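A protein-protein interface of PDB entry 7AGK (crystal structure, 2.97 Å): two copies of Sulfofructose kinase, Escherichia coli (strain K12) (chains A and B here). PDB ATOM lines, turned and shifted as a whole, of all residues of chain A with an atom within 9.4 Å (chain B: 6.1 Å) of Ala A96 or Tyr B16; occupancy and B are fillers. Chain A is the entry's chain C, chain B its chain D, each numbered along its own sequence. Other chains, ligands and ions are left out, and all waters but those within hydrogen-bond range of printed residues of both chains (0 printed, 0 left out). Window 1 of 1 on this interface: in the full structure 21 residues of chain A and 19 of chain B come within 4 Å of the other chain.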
ATOM      1  N   VAL A  11      -5.016 -21.848 -28.993  1.00  0.00           N
ATOM      2  CA  VAL A  11      -5.173 -22.482 -27.649  1.00  0.00           C
ATOM      3  C   VAL A  11      -4.279 -23.722 -27.591  1.00  0.00           C
ATOM      4  O   VAL A  11      -4.041 -24.339 -28.643  1.00  0.00           O
ATOM      5  CB  VAL A  11      -6.638 -22.863 -27.347  1.00  0.00           C
ATOM      6  CG1 VAL A  11      -7.625 -21.760 -27.689  1.00  0.00           C
ATOM      7  CG2 VAL A  11      -7.050 -24.149 -28.029  1.00  0.00           C
ATOM      8  N   MET A  12      -3.848 -24.122 -26.400  1.00  0.00           N
ATOM      9  CA  MET A  12      -3.177 -25.437 -26.233  1.00  0.00           C
ATOM     10  C   MET A  12      -4.273 -26.483 -26.003  1.00  0.00           C
ATOM     11  O   MET A  12      -5.010 -26.384 -25.002  1.00  0.00           O
ATOM     12  CB  MET A  12      -2.174 -25.440 -25.079  1.00  0.00           C
ATOM     13  N   ASP A  13      -4.416 -27.419 -26.939  1.00  0.00           N
ATOM     14  CA  ASP A  13      -5.336 -28.577 -26.813  1.00  0.00           C
ATOM     15  C   ASP A  13      -4.666 -29.592 -25.884  1.00  0.00           C
ATOM     16  O   ASP A  13      -3.490 -29.910 -26.086  1.00  0.00           O
ATOM     17  CB  ASP A  13      -5.721 -29.138 -28.187  1.00  0.00           C
ATOM     18  CG  ASP A  13      -6.710 -28.265 -28.963  1.00  0.00           C
ATOM     19  OD1 ASP A  13      -7.266 -27.318 -28.352  1.00  0.00           O
ATOM     20  OD2 ASP A  13      -6.925 -28.538 -30.173  1.00  0.00           O
ATOM     21  N   ARG A  14      -5.384 -30.010 -24.848  1.00  0.00           N
ATOM     22  CA  ARG A  14      -5.003 -31.111 -23.926  1.00  0.00           C
ATOM     23  C   ARG A  14      -5.898 -32.304 -24.272  1.00  0.00           C
ATOM     24  O   ARG A  14      -7.038 -32.323 -23.820  1.00  0.00           O
ATOM     25  CB  ARG A  14      -5.156 -30.658 -22.470  1.00  0.00           C
ATOM     26  N   ILE A  15      -5.380 -33.228 -25.076  1.00  0.00           N
ATOM     27  CA  ILE A  15      -6.152 -34.325 -25.724  1.00  0.00           C
ATOM     28  C   ILE A  15      -6.059 -35.566 -24.825  1.00  0.00           C
ATOM     29  O   ILE A  15      -4.927 -36.036 -24.560  1.00  0.00           O
ATOM     30  CB  ILE A  15      -5.612 -34.569 -27.152  1.00  0.00           C
ATOM     31  CG1 ILE A  15      -5.511 -33.274 -27.974  1.00  0.00           C
ATOM     32  CG2 ILE A  15      -6.423 -35.658 -27.846  1.00  0.00           C
ATOM     33  CD1 ILE A  15      -6.746 -32.924 -28.797  1.00  0.00           C
ATOM     34  N   TYR A  16      -7.207 -36.052 -24.348  1.00  0.00           N
ATOM     35  CA  TYR A  16      -7.341 -37.300 -23.547  1.00  0.00           C
ATOM     36  C   TYR A  16      -8.069 -38.357 -24.384  1.00  0.00           C
ATOM     37  O   TYR A  16      -9.266 -38.144 -24.685  1.00  0.00           O
ATOM     38  CB  TYR A  16      -8.135 -37.052 -22.263  1.00  0.00           C
ATOM     39  CG  TYR A  16      -7.523 -36.064 -21.308  1.00  0.00           C
ATOM     40  CD1 TYR A  16      -7.686 -34.703 -21.475  1.00  0.00           C
ATOM     41  CD2 TYR A  16      -6.788 -36.490 -20.220  1.00  0.00           C
ATOM     42  CE1 TYR A  16      -7.133 -33.788 -20.594  1.00  0.00           C
ATOM     43  CE2 TYR A  16      -6.227 -35.590 -19.326  1.00  0.00           C
ATOM     44  CZ  TYR A  16      -6.397 -34.229 -19.514  1.00  0.00           C
ATOM     45  OH  TYR A  16      -5.847 -33.323 -18.645  1.00  0.00           O
ATOM     46  N   TYR A  17      -7.382 -39.445 -24.743  1.00  0.00           N
ATOM     47  CA  TYR A  17      -7.965 -40.579 -25.504  1.00  0.00           C
ATOM     48  C   TYR A  17      -8.551 -41.578 -24.505  1.00  0.00           C
ATOM     49  O   TYR A  17      -7.780 -42.102 -23.695  1.00  0.00           O
ATOM     50  CB  TYR A  17      -6.930 -41.221 -26.429  1.00  0.00           C
ATOM     51  CG  TYR A  17      -6.287 -40.267 -27.402  1.00  0.00           C
ATOM     52  CD1 TYR A  17      -6.870 -39.989 -28.633  1.00  0.00           C
ATOM     53  CD2 TYR A  17      -5.087 -39.649 -27.088  1.00  0.00           C
ATOM     54  CE1 TYR A  17      -6.281 -39.112 -29.528  1.00  0.00           C
ATOM     55  CE2 TYR A  17      -4.482 -38.775 -27.983  1.00  0.00           C
ATOM     56  CZ  TYR A  17      -5.074 -38.510 -29.209  1.00  0.00           C
ATOM     57  OH  TYR A  17      -4.477 -37.634 -30.072  1.00  0.00           O
ATOM     58  N   TYR A  33      -2.658 -39.521 -23.654  1.00  0.00           N
ATOM     59  CA  TYR A  33      -2.704 -38.040 -23.562  1.00  0.00           C
ATOM     60  C   TYR A  33      -1.643 -37.410 -24.471  1.00  0.00           C
ATOM     61  O   TYR A  33      -0.519 -37.940 -24.544  1.00  0.00           O
ATOM     62  CB  TYR A  33      -2.458 -37.594 -22.115  1.00  0.00           C
ATOM     63  CG  TYR A  33      -2.415 -36.095 -21.919  1.00  0.00           C
ATOM     64  CD1 TYR A  33      -3.566 -35.332 -21.979  1.00  0.00           C
ATOM     65  CD2 TYR A  33      -1.221 -35.430 -21.690  1.00  0.00           C
ATOM     66  CE1 TYR A  33      -3.545 -33.956 -21.807  1.00  0.00           C
ATOM     67  CE2 TYR A  33      -1.175 -34.053 -21.536  1.00  0.00           C
ATOM     68  CZ  TYR A  33      -2.341 -33.308 -21.587  1.00  0.00           C
ATOM     69  OH  TYR A  33      -2.284 -31.952 -21.424  1.00  0.00           O
ATOM     70  N   THR A  34      -1.991 -36.300 -25.124  1.00  0.00           N
ATOM     71  CA  THR A  34      -1.045 -35.414 -25.853  1.00  0.00           C
ATOM     72  C   THR A  34      -1.468 -33.947 -25.673  1.00  0.00           C
ATOM     73  O   THR A  34      -2.675 -33.662 -25.577  1.00  0.00           O
ATOM     74  CB  THR A  34      -0.926 -35.791 -27.338  1.00  0.00           C
ATOM     75  OG1 THR A  34      -2.223 -35.738 -27.940  1.00  0.00           O
ATOM     76  CG2 THR A  34      -0.293 -37.150 -27.529  1.00  0.00           C
ATOM     77  N   VAL A  36      -1.091 -30.684 -27.828  1.00  0.00           N
ATOM     78  CA  VAL A  36      -0.867 -30.200 -29.223  1.00  0.00           C
ATOM     79  C   VAL A  36      -1.523 -28.817 -29.338  1.00  0.00           C
ATOM     80  O   VAL A  36      -2.575 -28.612 -28.733  1.00  0.00           O
ATOM     81  CB  VAL A  36      -1.466 -31.195 -30.238  1.00  0.00           C
ATOM     82  CG1 VAL A  36      -1.059 -32.644 -29.992  1.00  0.00           C
ATOM     83  CG2 VAL A  36      -2.986 -31.098 -30.292  1.00  0.00           C
ATOM     84  N   SER A  92      -2.181 -17.847 -21.579  1.00  0.00           N
ATOM     85  CA  SER A  92      -2.861 -18.144 -22.868  1.00  0.00           C
ATOM     86  C   SER A  92      -4.090 -19.030 -22.599  1.00  0.00           C
ATOM     87  O   SER A  92      -4.196 -19.568 -21.470  1.00  0.00           O
ATOM     88  CB  SER A  92      -1.906 -18.807 -23.837  1.00  0.00           C
ATOM     89  OG  SER A  92      -0.577 -18.337 -23.657  1.00  0.00           O
ATOM     90  N   SER A  93      -4.973 -19.180 -23.595  1.00  0.00           N
ATOM     91  CA  SER A  93      -6.211 -19.999 -23.524  1.00  0.00           C
ATOM     92  C   SER A  93      -5.862 -21.476 -23.701  1.00  0.00           C
ATOM     93  O   SER A  93      -4.775 -21.758 -24.194  1.00  0.00           O
ATOM     94  CB  SER A  93      -7.209 -19.540 -24.552  1.00  0.00           C
ATOM     95  OG  SER A  93      -7.683 -18.239 -24.242  1.00  0.00           O
ATOM     96  N   GLN A  94      -6.765 -22.378 -23.333  1.00  0.00           N
ATOM     97  CA  GLN A  94      -6.534 -23.845 -23.388  1.00  0.00           C
ATOM     98  C   GLN A  94      -7.881 -24.564 -23.506  1.00  0.00           C
ATOM     99  O   GLN A  94      -8.906 -23.956 -23.139  1.00  0.00           O
ATOM    100  CB  GLN A  94      -5.888 -24.303 -22.081  1.00  0.00           C
ATOM    101  CG  GLN A  94      -6.933 -24.687 -21.035  1.00  0.00           C
ATOM    102  CD  GLN A  94      -6.313 -25.145 -19.747  1.00  0.00           C
ATOM    103  OE1 GLN A  94      -6.025 -26.327 -19.560  1.00  0.00           O
ATOM    104  NE2 GLN A  94      -6.082 -24.196 -18.854  1.00  0.00           N
ATOM    105  N   SER A  95      -7.859 -25.834 -23.907  1.00  0.00           N
ATOM    106  CA  SER A  95      -9.042 -26.732 -23.945  1.00  0.00           C
ATOM    107  C   SER A  95      -8.640 -28.124 -23.471  1.00  0.00           C
ATOM    108  O   SER A  95      -7.554 -28.591 -23.857  1.00  0.00           O
ATOM    109  CB  SER A  95      -9.628 -26.805 -25.325  1.00  0.00           C
ATOM    110  OG  SER A  95      -9.853 -25.509 -25.845  1.00  0.00           O
ATOM    111  N   ALA A  96      -9.492 -28.756 -22.671  1.00  0.00           N
ATOM    112  CA  ALA A  96      -9.465 -30.213 -22.416  1.00  0.00           C
ATOM    113  C   ALA A  96     -10.333 -30.879 -23.475  1.00  0.00           C
ATOM    114  O   ALA A  96     -11.475 -30.429 -23.664  1.00  0.00           O
ATOM    115  CB  ALA A  96      -9.952 -30.538 -21.027  1.00  0.00           C
ATOM    116  N   ILE A  97      -9.786 -31.881 -24.156  1.00  0.00           N
ATOM    117  CA  ILE A  97     -10.506 -32.652 -25.203  1.00  0.00           C
ATOM    118  C   ILE A  97     -10.469 -34.129 -24.824  1.00  0.00           C
ATOM    119  O   ILE A  97      -9.364 -34.648 -24.573  1.00  0.00           O
ATOM    120  CB  ILE A  97      -9.899 -32.388 -26.590  1.00  0.00           C
ATOM    121  CG1 ILE A  97      -9.931 -30.894 -26.923  1.00  0.00           C
ATOM    122  CG2 ILE A  97     -10.599 -33.242 -27.637  1.00  0.00           C
ATOM    123  CD1 ILE A  97      -9.432 -30.549 -28.305  1.00  0.00           C
ATOM    124  N   MET A  98     -11.649 -34.748 -24.785  1.00  0.00           N
ATOM    125  CA  MET A  98     -11.832 -36.215 -24.667  1.00  0.00           C
ATOM    126  C   MET A  98     -12.177 -36.771 -26.059  1.00  0.00           C
ATOM    127  O   MET A  98     -13.031 -36.179 -26.747  1.00  0.00           O
ATOM    128  CB  MET A  98     -12.938 -36.537 -23.660  1.00  0.00           C
ATOM    129  N   VAL A  99     -11.517 -37.860 -26.452  1.00  0.00           N
ATOM    130  CA  VAL A  99     -11.580 -38.450 -27.821  1.00  0.00           C
ATOM    131  C   VAL A  99     -11.869 -39.945 -27.695  1.00  0.00           C
ATOM    132  O   VAL A  99     -11.019 -40.655 -27.106  1.00  0.00           O
ATOM    133  CB  VAL A  99     -10.255 -38.222 -28.559  1.00  0.00           C
ATOM    134  CG1 VAL A  99     -10.292 -38.836 -29.948  1.00  0.00           C
ATOM    135  CG2 VAL A  99      -9.893 -36.747 -28.597  1.00  0.00           C
ATOM    136  N   ARG A 105     -15.252 -36.379 -30.545  1.00  0.00           N
ATOM    137  CA  ARG A 105     -14.519 -35.539 -29.552  1.00  0.00           C
ATOM    138  C   ARG A 105     -15.486 -34.629 -28.785  1.00  0.00           C
ATOM    139  O   ARG A 105     -16.415 -34.079 -29.399  1.00  0.00           O
ATOM    140  CB  ARG A 105     -13.382 -34.712 -30.177  1.00  0.00           C
ATOM    141  CG  ARG A 105     -13.514 -34.383 -31.648  1.00  0.00           C
ATOM    142  CD  ARG A 105     -12.148 -33.942 -32.117  1.00  0.00           C
ATOM    143  NE  ARG A 105     -11.190 -35.042 -32.134  1.00  0.00           N
ATOM    144  CZ  ARG A 105      -9.880 -34.882 -32.264  1.00  0.00           C
ATOM    145  NH1 ARG A 105      -9.373 -33.662 -32.363  1.00  0.00           N
ATOM    146  NH2 ARG A 105      -9.079 -35.934 -32.274  1.00  0.00           N
ATOM    147  N   ILE A 106     -15.272 -34.501 -27.472  1.00  0.00           N
ATOM    148  CA  ILE A 106     -15.866 -33.439 -26.611  1.00  0.00           C
ATOM    149  C   ILE A 106     -14.763 -32.438 -26.262  1.00  0.00           C
ATOM    150  O   ILE A 106     -13.753 -32.869 -25.715  1.00  0.00           O
ATOM    151  CB  ILE A 106     -16.478 -34.027 -25.332  1.00  0.00           C
ATOM    152  CG1 ILE A 106     -17.426 -35.196 -25.653  1.00  0.00           C
ATOM    153  CG2 ILE A 106     -17.088 -32.880 -24.535  1.00  0.00           C
ATOM    154  CD1 ILE A 106     -18.415 -35.581 -24.578  1.00  0.00           C
ATOM    155  N   ILE A 107     -14.958 -31.161 -26.582  1.00  0.00           N
ATOM    156  CA  ILE A 107     -13.954 -30.071 -26.390  1.00  0.00           C
ATOM    157  C   ILE A 107     -14.512 -29.086 -25.359  1.00  0.00           C
ATOM    158  O   ILE A 107     -15.646 -28.610 -25.553  1.00  0.00           O
ATOM    159  CB  ILE A 107     -13.614 -29.372 -27.718  1.00  0.00           C
ATOM    160  N   ILE A 108     -13.771 -28.871 -24.270  1.00  0.00           N
ATOM    161  CA  ILE A 108     -14.138 -27.951 -23.158  1.00  0.00           C
ATOM    162  C   ILE A 108     -13.060 -26.860 -23.110  1.00  0.00           C
ATOM    163  O   ILE A 108     -11.894 -27.123 -22.735  1.00  0.00           O
ATOM    164  CB  ILE A 108     -14.342 -28.703 -21.831  1.00  0.00           C
ATOM    165  CG1 ILE A 108     -14.741 -27.744 -20.712  1.00  0.00           C
ATOM    166  CG2 ILE A 108     -13.140 -29.545 -21.484  1.00  0.00           C
ATOM    167  CD1 ILE A 108     -16.044 -27.012 -20.971  1.00  0.00           C
ATOM    168  N   ASN A 109     -13.430 -25.697 -23.629  1.00  0.00           N
ATOM    169  CA  ASN A 109     -12.506 -24.563 -23.892  1.00  0.00           C
ATOM    170  C   ASN A 109     -12.548 -23.646 -22.681  1.00  0.00           C
ATOM    171  O   ASN A 109     -13.656 -23.422 -22.187  1.00  0.00           O
ATOM    172  CB  ASN A 109     -12.890 -23.778 -25.148  1.00  0.00           C
ATOM    173  CG  ASN A 109     -12.191 -22.442 -25.225  1.00  0.00           C
ATOM    174  OD1 ASN A 109     -12.835 -21.402 -25.296  1.00  0.00           O
ATOM    175  ND2 ASN A 109     -10.874 -22.457 -25.187  1.00  0.00           N
ATOM    176  N   TYR A 110     -11.390 -23.166 -22.232  1.00  0.00           N
ATOM    177  CA  TYR A 110     -11.266 -22.070 -21.233  1.00  0.00           C
ATOM    178  C   TYR A 110     -10.576 -20.881 -21.892  1.00  0.00           C
ATOM    179  O   TYR A 110      -9.365 -20.906 -22.121  1.00  0.00           O
ATOM    180  CB  TYR A 110     -10.511 -22.478 -19.964  1.00  0.00           C
ATOM    181  CG  TYR A 110     -10.498 -21.371 -18.938  1.00  0.00           C
ATOM    182  CD1 TYR A 110     -11.681 -20.903 -18.385  1.00  0.00           C
ATOM    183  CD2 TYR A 110      -9.320 -20.740 -18.567  1.00  0.00           C
ATOM    184  CE1 TYR A 110     -11.693 -19.859 -17.472  1.00  0.00           C
ATOM    185  CE2 TYR A 110      -9.314 -19.695 -17.653  1.00  0.00           C
ATOM    186  CZ  TYR A 110     -10.505 -19.253 -17.100  1.00  0.00           C
ATOM    187  OH  TYR A 110     -10.520 -18.223 -16.204  1.00  0.00           O
ATOM    188  N   PRO A 111     -11.343 -19.830 -22.253  1.00  0.00           N
ATOM    189  CA  PRO A 111     -10.756 -18.569 -22.701  1.00  0.00           C
ATOM    190  C   PRO A 111     -10.071 -17.835 -21.544  1.00  0.00           C
ATOM    191  O   PRO A 111     -10.749 -17.546 -20.581  1.00  0.00           O
ATOM    192  CB  PRO A 111     -11.968 -17.764 -23.190  1.00  0.00           C
ATOM    193  CG  PRO A 111     -13.145 -18.350 -22.418  1.00  0.00           C
ATOM    194  CD  PRO A 111     -12.814 -19.819 -22.270  1.00  0.00           C
ATOM    195  N   ARG B  14      -6.909 -30.625 -12.867  1.00  0.00           N
ATOM    196  CA  ARG B  14      -7.247 -29.459 -13.741  1.00  0.00           C
ATOM    197  C   ARG B  14      -8.767 -29.291 -13.738  1.00  0.00           C
ATOM    198  O   ARG B  14      -9.453 -30.039 -14.477  1.00  0.00           O
ATOM    199  CB  ARG B  14      -6.728 -29.688 -15.162  1.00  0.00           C
ATOM    200  CG  ARG B  14      -5.267 -30.091 -15.187  1.00  0.00           C
ATOM    201  CD  ARG B  14      -4.650 -29.692 -16.504  1.00  0.00           C
ATOM    202  NE  ARG B  14      -3.580 -30.593 -16.868  1.00  0.00           N
ATOM    203  CZ  ARG B  14      -3.155 -30.769 -18.101  1.00  0.00           C
ATOM    204  NH1 ARG B  14      -3.672 -30.045 -19.084  1.00  0.00           N
ATOM    205  NH2 ARG B  14      -2.166 -31.606 -18.339  1.00  0.00           N
ATOM    206  N   ILE B  15      -9.258 -28.381 -12.896  1.00  0.00           N
ATOM    207  CA  ILE B  15     -10.712 -28.230 -12.577  1.00  0.00           C
ATOM    208  C   ILE B  15     -11.334 -27.196 -13.533  1.00  0.00           C
ATOM    209  O   ILE B  15     -10.871 -26.042 -13.563  1.00  0.00           O
ATOM    210  CB  ILE B  15     -10.910 -27.877 -11.085  1.00  0.00           C
ATOM    211  N   TYR B  16     -12.337 -27.618 -14.308  1.00  0.00           N
ATOM    212  CA  TYR B  16     -13.154 -26.772 -15.218  1.00  0.00           C
ATOM    213  C   TYR B  16     -14.562 -26.625 -14.639  1.00  0.00           C
ATOM    214  O   TYR B  16     -15.261 -27.633 -14.542  1.00  0.00           O
ATOM    215  CB  TYR B  16     -13.233 -27.394 -16.616  1.00  0.00           C
ATOM    216  CG  TYR B  16     -11.905 -27.506 -17.327  1.00  0.00           C
ATOM    217  CD1 TYR B  16     -11.048 -28.575 -17.097  1.00  0.00           C
ATOM    218  CD2 TYR B  16     -11.492 -26.529 -18.225  1.00  0.00           C
ATOM    219  CE1 TYR B  16      -9.823 -28.671 -17.740  1.00  0.00           C
ATOM    220  CE2 TYR B  16     -10.269 -26.602 -18.866  1.00  0.00           C
ATOM    221  CZ  TYR B  16      -9.435 -27.680 -18.638  1.00  0.00           C
ATOM    222  OH  TYR B  16      -8.235 -27.695 -19.299  1.00  0.00           O
ATOM    223  N   TYR B  17     -14.964 -25.408 -14.264  1.00  0.00           N
ATOM    224  CA  TYR B  17     -16.342 -25.102 -13.784  1.00  0.00           C
ATOM    225  C   TYR B  17     -17.209 -24.752 -15.002  1.00  0.00           C
ATOM    226  O   TYR B  17     -16.855 -23.796 -15.750  1.00  0.00           O
ATOM    227  CB  TYR B  17     -16.330 -23.988 -12.740  1.00  0.00           C
ATOM    228  CG  TYR B  17     -15.438 -24.243 -11.549  1.00  0.00           C
ATOM    229  CD1 TYR B  17     -15.876 -24.965 -10.439  1.00  0.00           C
ATOM    230  CD2 TYR B  17     -14.142 -23.756 -11.532  1.00  0.00           C
ATOM    231  CE1 TYR B  17     -15.047 -25.180  -9.345  1.00  0.00           C
ATOM    232  CE2 TYR B  17     -13.304 -23.964 -10.446  1.00  0.00           C
ATOM    233  CZ  TYR B  17     -13.757 -24.682  -9.352  1.00  0.00           C
ATOM    234  OH  TYR B  17     -12.947 -24.902  -8.280  1.00  0.00           O
ATOM    235  N   VAL B  18     -18.271 -25.536 -15.216  1.00  0.00           N
ATOM    236  CA  VAL B  18     -19.109 -25.521 -16.451  1.00  0.00           C
ATOM    237  C   VAL B  18     -20.557 -25.267 -16.032  1.00  0.00           C
ATOM    238  O   VAL B  18     -20.859 -25.477 -14.856  1.00  0.00           O
ATOM    239  CB  VAL B  18     -18.973 -26.831 -17.248  1.00  0.00           C
ATOM    240  N   ALA B  30     -15.906 -23.395 -20.469  1.00  0.00           N
ATOM    241  CA  ALA B  30     -15.850 -23.330 -18.992  1.00  0.00           C
ATOM    242  C   ALA B  30     -15.953 -21.867 -18.562  1.00  0.00           C
ATOM    243  O   ALA B  30     -15.207 -21.010 -19.136  1.00  0.00           O
ATOM    244  CB  ALA B  30     -14.567 -23.946 -18.495  1.00  0.00           C
ATOM    245  N   ASN B  32     -15.009 -20.982 -15.616  1.00  0.00           N
ATOM    246  CA  ASN B  32     -13.808 -20.768 -14.754  1.00  0.00           C
ATOM    247  C   ASN B  32     -12.933 -22.032 -14.657  1.00  0.00           C
ATOM    248  O   ASN B  32     -13.436 -23.132 -14.970  1.00  0.00           O
ATOM    249  CB  ASN B  32     -14.223 -20.289 -13.362  1.00  0.00           C
ATOM    250  CG  ASN B  32     -13.198 -19.377 -12.725  1.00  0.00           C
ATOM    251  OD1 ASN B  32     -12.495 -18.647 -13.415  1.00  0.00           O
ATOM    252  ND2 ASN B  32     -13.105 -19.406 -11.408  1.00  0.00           N
ATOM    253  N   TYR B  33     -11.670 -21.874 -14.226  1.00  0.00           N
ATOM    254  CA  TYR B  33     -10.619 -22.932 -14.195  1.00  0.00           C
ATOM    255  C   TYR B  33      -9.677 -22.732 -13.000  1.00  0.00           C
ATOM    256  O   TYR B  33      -9.337 -21.584 -12.697  1.00  0.00           O
ATOM    257  CB  TYR B  33      -9.802 -22.916 -15.492  1.00  0.00           C
ATOM    258  CG  TYR B  33      -8.662 -23.903 -15.534  1.00  0.00           C
ATOM    259  CD1 TYR B  33      -8.887 -25.263 -15.655  1.00  0.00           C
ATOM    260  CD2 TYR B  33      -7.349 -23.476 -15.435  1.00  0.00           C
ATOM    261  CE1 TYR B  33      -7.848 -26.178 -15.681  1.00  0.00           C
ATOM    262  CE2 TYR B  33      -6.294 -24.375 -15.462  1.00  0.00           C
ATOM    263  CZ  TYR B  33      -6.542 -25.733 -15.572  1.00  0.00           C
ATOM    264  OH  TYR B  33      -5.498 -26.619 -15.590  1.00  0.00           O
ATOM    265  N   THR B  34      -9.259 -23.829 -12.359  1.00  0.00           N
ATOM    266  CA  THR B  34      -8.283 -23.863 -11.238  1.00  0.00           C
ATOM    267  C   THR B  34      -7.429 -25.138 -11.347  1.00  0.00           C
ATOM    268  O   THR B  34      -7.944 -26.191 -11.809  1.00  0.00           O
ATOM    269  CB  THR B  34      -9.006 -23.772  -9.887  1.00  0.00           C
ATOM    270  N   ALA B  96      -8.293 -34.129 -15.944  1.00  0.00           N
ATOM    271  CA  ALA B  96      -9.248 -33.057 -16.285  1.00  0.00           C
ATOM    272  C   ALA B  96     -10.539 -33.339 -15.524  1.00  0.00           C
ATOM    273  O   ALA B  96     -11.030 -34.481 -15.584  1.00  0.00           O
ATOM    274  CB  ALA B  96      -9.475 -32.997 -17.769  1.00  0.00           C
ATOM    275  N   ILE B  97     -11.044 -32.343 -14.802  1.00  0.00           N
ATOM    276  CA  ILE B  97     -12.316 -32.451 -14.035  1.00  0.00           C
ATOM    277  C   ILE B  97     -13.251 -31.321 -14.468  1.00  0.00           C
ATOM    278  O   ILE B  97     -12.819 -30.161 -14.468  1.00  0.00           O
ATOM    279  CB  ILE B  97     -12.035 -32.419 -12.524  1.00  0.00           C
ATOM    280  CG1 ILE B  97     -11.078 -33.537 -12.111  1.00  0.00           C
ATOM    281  CG2 ILE B  97     -13.329 -32.491 -11.748  1.00  0.00           C
ATOM    282  CD1 ILE B  97     -10.622 -33.465 -10.679  1.00  0.00           C
ATOM    283  N   MET B  98     -14.485 -31.674 -14.822  1.00  0.00           N
ATOM    284  CA  MET B  98     -15.621 -30.750 -15.052  1.00  0.00           C
ATOM    285  C   MET B  98     -16.537 -30.779 -13.811  1.00  0.00           C
ATOM    286  O   MET B  98     -16.827 -31.889 -13.299  1.00  0.00           O
ATOM    287  CB  MET B  98     -16.382 -31.174 -16.315  1.00  0.00           C
ATOM    288  N   VAL B  99     -16.978 -29.600 -13.365  1.00  0.00           N
ATOM    289  CA  VAL B  99     -17.775 -29.386 -12.122  1.00  0.00           C
ATOM    290  C   VAL B  99     -19.001 -28.529 -12.457  1.00  0.00           C
ATOM    291  O   VAL B  99     -18.795 -27.360 -12.875  1.00  0.00           O
ATOM    292  CB  VAL B  99     -16.905 -28.697 -11.055  1.00  0.00           C
ATOM    293  N   ASP B 100     -20.210 -29.080 -12.276  1.00  0.00           N
ATOM    294  CA  ASP B 100     -21.518 -28.422 -12.570  1.00  0.00           C
ATOM    295  C   ASP B 100     -21.797 -27.395 -11.471  1.00  0.00           C
ATOM    296  O   ASP B 100     -21.058 -27.409 -10.457  1.00  0.00           O
ATOM    297  CB  ASP B 100     -22.677 -29.425 -12.698  1.00  0.00           C
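Arg B14 touches Arg A14. Arg B14 touches Tyr A16 (CZ to OH, 3.8 Å). Tyr A16 touches Ala B96. CE2 of Tyr B33 touches NE2 of Gln A94, at 3.4 Å. Ala A96 touches Tyr B16 (CB to OH, 3.7 Å). N of Ala B30 touches CD1 of Ile A108, 3.7 Å away. Ala B30 touches Tyr A110 (O to CD1, 3.6 Å). Tyr B33 touches Tyr A110 (CB to CD2, 3.8 Å).
Ala A96 touches just one residue of chain B: Tyr B16 (3.7 Å). Of the printed residues of chain A, Tyr B16 touches Gln A94 and Ala A96. No residue of chain A comes within 4 Å of Ile B15. No residue of chain A comes within 4 Å of Met B98. No residue of chain A comes within 4 Å of Val B99. Of the printed residues of chain A, Arg B14 touches Arg A14, Tyr A16 and Tyr A33. Of the printed residues of chain B, Tyr A16 touches Arg B14 (3.8 Å) and Ala B96 (3.7 Å). Of the printed residues of chain B, Gln A94 touches Tyr B16 and Tyr B33. Of the printed residues of chain B, Asn A109 touches Ala B30 (2.8 Å). Asp A13 touches none of the printed residues of chain B. The nearest residue of chain B that does not touch Ala A96 is Ala B96 (4.1 Å). The nearest printed residue of chain A that does not touch Tyr B16 is Ser A95 (4.2 Å). The nearest printed residue of chain B that does not touch Tyr A16 is Tyr B16 (6.1 Å).
Arg A14 touches its own counterpart, Arg B14. Tyr A16 touches Arg B14, but with the chains exchanged Arg A14 does not touch Tyr B16 (5.3 Å). Tyr A16 touches Ala B96, and with the chains exchanged Ala A96 touches Tyr B16. Tyr A33 touches Arg B14, but with the chains exchanged Arg A14 does not touch Tyr B33 (8.0 Å). 10 positions are printed for both chains.
The guanidinium group (NH2) of Arg B14 lies within hydrogen-bond range of the side-chain hydroxyl (OH) of Tyr A33 (3.1 Å). OH of Tyr B16 sits at hydrogen-bond distance from OE1 of Gln A94 (2.6 Å). N of Ala B30 sits at hydrogen-bond distance from O of Asn A109 (2.8 Å). The side-chain amide oxygen (OD1) of Asn B32 lies within hydrogen-bond range of the side-chain hydroxyl (OH) of Tyr A110 (3.4 Å).
N of Tyr B16 is in hydrogen-bond range of O of Ile B97, at 2.6 Å. The backbone carbonyl oxygen of Ser A95 sits at hydrogen-bond distance from the backbone NH of Arg A14. N of Ile A97 lies within hydrogen-bond range of O of Arg A14, 2.8 Å away. The backbone NH (N) of Val A99 lies within hydrogen-bond range of the backbone carbonyl oxygen (O) of Tyr A16 (2.9 Å). The backbone NH (N) of Tyr A110 lies within hydrogen-bond range of the backbone carbonyl oxygen (O) of Gln A94 (2.8 Å). The backbone carbonyl oxygen (O) of Ala A96 is in hydrogen-bond range of the backbone NH (N) of Ile A108 (2.8 Å).
Of the 25 printed residues of chain A, 8 touch a printed residue of chain B. Printed residues of chain A that touch a printed residue of chain B: Arg A14, Tyr A16, Tyr A33, Gln A94, Ala A96, Ile A108, Asn A109 and Tyr A110. Of the 14 printed residues of chain B, 6 touch a printed residue of chain A. Among the printed residues, 12 pairs touch across the chains.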
